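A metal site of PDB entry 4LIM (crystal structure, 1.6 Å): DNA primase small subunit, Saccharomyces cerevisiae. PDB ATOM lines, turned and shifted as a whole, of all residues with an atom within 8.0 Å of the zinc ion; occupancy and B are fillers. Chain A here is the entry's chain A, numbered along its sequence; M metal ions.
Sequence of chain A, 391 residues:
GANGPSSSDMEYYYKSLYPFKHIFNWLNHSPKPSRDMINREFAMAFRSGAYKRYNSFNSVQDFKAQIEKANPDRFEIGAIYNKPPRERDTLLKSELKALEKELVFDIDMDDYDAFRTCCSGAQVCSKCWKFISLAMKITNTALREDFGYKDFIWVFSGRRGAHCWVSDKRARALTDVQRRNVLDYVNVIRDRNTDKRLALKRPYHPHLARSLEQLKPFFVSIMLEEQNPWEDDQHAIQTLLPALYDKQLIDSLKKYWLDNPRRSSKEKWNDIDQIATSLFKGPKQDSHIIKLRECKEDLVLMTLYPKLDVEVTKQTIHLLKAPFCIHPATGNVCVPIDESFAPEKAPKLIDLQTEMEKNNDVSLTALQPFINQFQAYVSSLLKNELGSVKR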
ATOM      1  N   MET A 109      35.168  27.167  16.280  1.00  0.00           N
ATOM      2  CA  MET A 109      34.497  28.084  17.193  1.00  0.00           C
ATOM      3  C   MET A 109      35.356  28.732  18.291  1.00  0.00           C
ATOM      4  O   MET A 109      35.076  29.876  18.690  1.00  0.00           O
ATOM      5  CB  MET A 109      33.343  27.344  17.841  1.00  0.00           C
ATOM      6  CG  MET A 109      32.558  28.240  18.745  1.00  0.00           C
ATOM      7  SD  MET A 109      31.464  29.204  17.725  1.00  0.00           S
ATOM      8  CE  MET A 109      30.267  27.962  17.790  1.00  0.00           C
ATOM      9  N   ARG A 116      30.361  35.038  22.815  1.00  0.00           N
ATOM     10  CA  ARG A 116      29.115  34.277  22.795  1.00  0.00           C
ATOM     11  C   ARG A 116      28.675  34.036  24.234  1.00  0.00           C
ATOM     12  O   ARG A 116      29.490  33.894  25.165  1.00  0.00           O
ATOM     13  CB  ARG A 116      29.221  32.981  21.960  1.00  0.00           C
ATOM     14  CG  ARG A 116      29.756  31.855  22.699  1.00  0.00           C
ATOM     15  CD  ARG A 116      29.855  30.578  21.865  1.00  0.00           C
ATOM     16  NE  ARG A 116      30.438  29.591  22.729  1.00  0.00           N
ATOM     17  CZ  ARG A 116      30.461  28.259  22.479  1.00  0.00           C
ATOM     18  NH1 ARG A 116      29.932  27.712  21.365  1.00  0.00           N
ATOM     19  NH2 ARG A 116      31.036  27.473  23.403  1.00  0.00           N
ATOM     20  N   THR A 117      27.361  34.033  24.381  1.00  0.00           N
ATOM     21  CA  THR A 117      26.744  33.732  25.658  1.00  0.00           C
ATOM     22  C   THR A 117      25.772  32.538  25.592  1.00  0.00           C
ATOM     23  O   THR A 117      25.287  32.046  26.652  1.00  0.00           O
ATOM     24  CB  THR A 117      25.960  34.928  26.167  1.00  0.00           C
ATOM     25  OG1 THR A 117      24.810  35.161  25.311  1.00  0.00           O
ATOM     26  CG2 THR A 117      26.868  36.195  26.272  1.00  0.00           C
ATOM     27  N   CYS A 118      25.370  32.164  24.390  1.00  0.00           N
ATOM     28  CA  CYS A 118      24.390  31.049  24.233  1.00  0.00           C
ATOM     29  C   CYS A 118      24.921  29.702  24.726  1.00  0.00           C
ATOM     30  O   CYS A 118      24.115  28.807  25.149  1.00  0.00           O
ATOM     31  CB  CYS A 118      24.022  30.851  22.731  1.00  0.00           C
ATOM     32  SG  CYS A 118      25.394  30.633  21.542  1.00  0.00           S
ATOM     33  N   CYS A 119      26.215  29.515  24.522  1.00  0.00           N
ATOM     34  CA  CYS A 119      26.939  28.244  24.791  1.00  0.00           C
ATOM     35  C   CYS A 119      28.178  28.555  25.614  1.00  0.00           C
ATOM     36  O   CYS A 119      28.672  29.687  25.597  1.00  0.00           O
ATOM     37  CB  CYS A 119      27.321  27.476  23.530  1.00  0.00           C
ATOM     38  SG  CYS A 119      25.788  26.862  22.652  1.00  0.00           S
ATOM     39  N   SER A 120      28.647  27.588  26.400  1.00  0.00           N
ATOM     40  CA  SER A 120      29.884  27.736  27.153  1.00  0.00           C
ATOM     41  C   SER A 120      30.703  26.456  26.966  1.00  0.00           C
ATOM     42  O   SER A 120      30.160  25.399  26.497  1.00  0.00           O
ATOM     43  CB  SER A 120      29.557  28.040  28.642  1.00  0.00           C
ATOM     44  OG  SER A 120      28.739  26.993  29.162  1.00  0.00           O
ATOM     45  N   GLN A 123      30.257  23.364  24.144  1.00  0.00           N
ATOM     46  CA  GLN A 123      28.932  23.475  23.514  1.00  0.00           C
ATOM     47  C   GLN A 123      28.906  24.155  22.204  1.00  0.00           C
ATOM     48  O   GLN A 123      29.787  24.996  21.907  1.00  0.00           O
ATOM     49  CB  GLN A 123      27.966  24.261  24.408  1.00  0.00           C
ATOM     50  CG  GLN A 123      27.617  23.517  25.723  1.00  0.00           C
ATOM     51  CD  GLN A 123      26.667  24.277  26.599  1.00  0.00           C
ATOM     52  OE1 GLN A 123      26.598  25.510  26.591  1.00  0.00           O
ATOM     53  NE2 GLN A 123      25.925  23.535  27.451  1.00  0.00           N
ATOM     54  N   VAL A 124      27.875  23.836  21.408  1.00  0.00           N
ATOM     55  CA  VAL A 124      27.583  24.612  20.197  1.00  0.00           C
ATOM     56  C   VAL A 124      26.059  24.531  19.958  1.00  0.00           C
ATOM     57  O   VAL A 124      25.381  23.579  20.461  1.00  0.00           O
ATOM     58  CB  VAL A 124      28.383  24.033  19.022  1.00  0.00           C
ATOM     59  CG1 VAL A 124      28.005  22.543  18.821  1.00  0.00           C
ATOM     60  CG2 VAL A 124      28.211  24.851  17.719  1.00  0.00           C
ATOM     61  N   CYS A 125      25.505  25.468  19.215  1.00  0.00           N
ATOM     62  CA  CYS A 125      24.086  25.509  18.874  1.00  0.00           C
ATOM     63  C   CYS A 125      23.914  26.328  17.602  1.00  0.00           C
ATOM     64  O   CYS A 125      24.870  26.860  17.089  1.00  0.00           O
ATOM     65  CB  CYS A 125      23.265  26.100  20.032  1.00  0.00           C
ATOM     66  SG  CYS A 125      23.426  27.958  20.228  1.00  0.00           S
ATOM     67  N   SER A 126      22.679  26.464  17.100  1.00  0.00           N
ATOM     68  CA  SER A 126      22.510  27.102  15.791  1.00  0.00           C
ATOM     69  C   SER A 126      22.753  28.593  15.925  1.00  0.00           C
ATOM     70  O   SER A 126      23.114  29.233  14.954  1.00  0.00           O
ATOM     71  CB  SER A 126      21.089  26.848  15.272  1.00  0.00           C
ATOM     72  OG  SER A 126      20.133  27.331  16.204  1.00  0.00           O
ATOM     73  N   LYS A 127      22.653  29.112  17.140  1.00  0.00           N
ATOM     74  CA  LYS A 127      22.944  30.547  17.296  1.00  0.00           C
ATOM     75  C   LYS A 127      24.436  30.871  17.135  1.00  0.00           C
ATOM     76  O   LYS A 127      24.799  31.795  16.352  1.00  0.00           O
ATOM     77  CB  LYS A 127      22.480  31.084  18.644  1.00  0.00           C
ATOM     78  CG  LYS A 127      20.963  30.966  18.902  1.00  0.00           C
ATOM     79  CD  LYS A 127      20.653  31.370  20.311  1.00  0.00           C
ATOM     80  CE  LYS A 127      19.191  31.147  20.651  1.00  0.00           C
ATOM     81  NZ  LYS A 127      18.961  31.273  22.124  1.00  0.00           N
ATOM     82  N   CYS A 128      25.324  30.186  17.878  1.00  0.00           N
ATOM     83  CA  CYS A 128      26.727  30.542  17.711  1.00  0.00           C
ATOM     84  C   CYS A 128      27.248  29.974  16.422  1.00  0.00           C
ATOM     85  O   CYS A 128      28.278  30.406  15.902  1.00  0.00           O
ATOM     86  CB  CYS A 128      27.621  30.137  18.877  1.00  0.00           C
ATOM     87  SG  CYS A 128      27.258  28.410  19.538  1.00  0.00           S
ATOM     88  N   TRP A 129      26.591  28.947  15.864  1.00  0.00           N
ATOM     89  CA  TRP A 129      26.982  28.522  14.533  1.00  0.00           C
ATOM     90  C   TRP A 129      26.976  29.654  13.497  1.00  0.00           C
ATOM     91  O   TRP A 129      27.760  29.588  12.537  1.00  0.00           O
ATOM     92  CB  TRP A 129      26.154  27.316  14.038  1.00  0.00           C
ATOM     93  CG  TRP A 129      26.698  26.725  12.743  1.00  0.00           C
ATOM     94  CD1 TRP A 129      26.138  26.813  11.490  1.00  0.00           C
ATOM     95  CD2 TRP A 129      27.893  25.947  12.584  1.00  0.00           C
ATOM     96  NE1 TRP A 129      26.949  26.203  10.560  1.00  0.00           N
ATOM     97  CE2 TRP A 129      28.029  25.650  11.201  1.00  0.00           C
ATOM     98  CE3 TRP A 129      28.921  25.542  13.488  1.00  0.00           C
ATOM     99  CZ2 TRP A 129      29.122  24.932  10.685  1.00  0.00           C
ATOM    100  CZ3 TRP A 129      29.997  24.796  12.953  1.00  0.00           C
ATOM    101  CH2 TRP A 129      30.087  24.504  11.597  1.00  0.00           C
ATOM    102  N   LYS A 130      26.155  30.690  13.723  1.00  0.00           N
ATOM    103  CA  LYS A 130      26.116  31.834  12.794  1.00  0.00           C
ATOM    104  C   LYS A 130      27.492  32.458  12.665  1.00  0.00           C
ATOM    105  O   LYS A 130      27.811  33.016  11.588  1.00  0.00           O
ATOM    106  CB  LYS A 130      25.108  32.901  13.214  1.00  0.00           C
ATOM    107  CG  LYS A 130      23.665  32.348  13.327  1.00  0.00           C
ATOM    108  CD  LYS A 130      22.691  33.440  13.782  1.00  0.00           C
ATOM    109  CE  LYS A 130      21.287  32.900  13.867  1.00  0.00           C
ATOM    110  NZ  LYS A 130      20.407  33.954  14.383  1.00  0.00           N
ATOM    111  N   PHE A 131      28.336  32.394  13.710  1.00  0.00           N
ATOM    112  CA  PHE A 131      29.725  32.905  13.574  1.00  0.00           C
ATOM    113  C   PHE A 131      30.478  32.151  12.462  1.00  0.00           C
ATOM    114  O   PHE A 131      31.196  32.747  11.640  1.00  0.00           O
ATOM    115  CB  PHE A 131      30.540  32.752  14.876  1.00  0.00           C
ATOM    116  CG  PHE A 131      30.111  33.670  15.987  1.00  0.00           C
ATOM    117  CD1 PHE A 131      30.394  35.021  15.919  1.00  0.00           C
ATOM    118  CD2 PHE A 131      29.528  33.165  17.140  1.00  0.00           C
ATOM    119  CE1 PHE A 131      30.051  35.892  16.939  1.00  0.00           C
ATOM    120  CE2 PHE A 131      29.148  34.045  18.190  1.00  0.00           C
ATOM    121  CZ  PHE A 131      29.404  35.417  18.083  1.00  0.00           C
ATOM    122  N   ARG A 160      32.415  21.640  16.137  1.00  0.00           N
ATOM    123  CA  ARG A 160      31.943  23.019  15.995  1.00  0.00           C
ATOM    124  C   ARG A 160      32.876  23.821  15.119  1.00  0.00           C
ATOM    125  O   ARG A 160      33.186  24.999  15.393  1.00  0.00           O
ATOM    126  CB  ARG A 160      31.721  23.667  17.342  1.00  0.00           C
ATOM    127  CG  ARG A 160      32.960  23.649  18.228  1.00  0.00           C
ATOM    128  CD  ARG A 160      32.568  24.097  19.624  1.00  0.00           C
ATOM    129  NE  ARG A 160      33.748  24.407  20.426  1.00  0.00           N
ATOM    130  CZ  ARG A 160      33.865  25.496  21.210  1.00  0.00           C
ATOM    131  NH1 ARG A 160      32.925  26.439  21.217  1.00  0.00           N
ATOM    132  NH2 ARG A 160      34.989  25.697  21.909  1.00  0.00           N
ATOM    133  N   GLN A 227      23.450  37.379  21.111  1.00  0.00           N
ATOM    134  CA  GLN A 227      24.533  37.070  22.043  1.00  0.00           C
ATOM    135  C   GLN A 227      24.628  38.055  23.233  1.00  0.00           C
ATOM    136  O   GLN A 227      24.675  37.614  24.394  1.00  0.00           O
ATOM    137  CB  GLN A 227      25.881  36.984  21.294  1.00  0.00           C
ATOM    138  CG  GLN A 227      25.920  35.860  20.252  1.00  0.00           C
ATOM    139  CD  GLN A 227      25.668  34.492  20.827  1.00  0.00           C
ATOM    140  OE1 GLN A 227      25.964  34.228  21.994  1.00  0.00           O
ATOM    141  NE2 GLN A 227      25.069  33.618  20.018  1.00  0.00           N
HETATM  142 ZN    ZN M   1      25.513  28.445  21.059  1.00  0.00          ZN
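Within 4 Å of the zinc ion: Cys 118, Cys 119, Cys 125 and Cys 128.
SG of Cys 118 is bound to the zinc ion (2.2 Å).
The zinc ion is bound by SG of Cys 119, 2.3 Å away.
SG of Cys 125 binds the zinc ion (2.3 Å).
The side-chain sulfur (SG) of Cys 128 is bound to the zinc ion.
The zinc ion has four donor atoms within binding distance.
OE1 of Gln 227 lies within hydrogen-bond range of N of Cys 118 (3.2 Å).
The backbone carbonyl oxygen (O) of Cys 119 lies within hydrogen-bond range of the guanidinium group (NE) of Arg 116 (3.4 Å).
N of Lys 127 lies close to SG of Cys 125.
The guanidinium group (NH1) of Arg 116 sits close to the side-chain sulfur (SG) of Cys 128 (3.3 Å).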
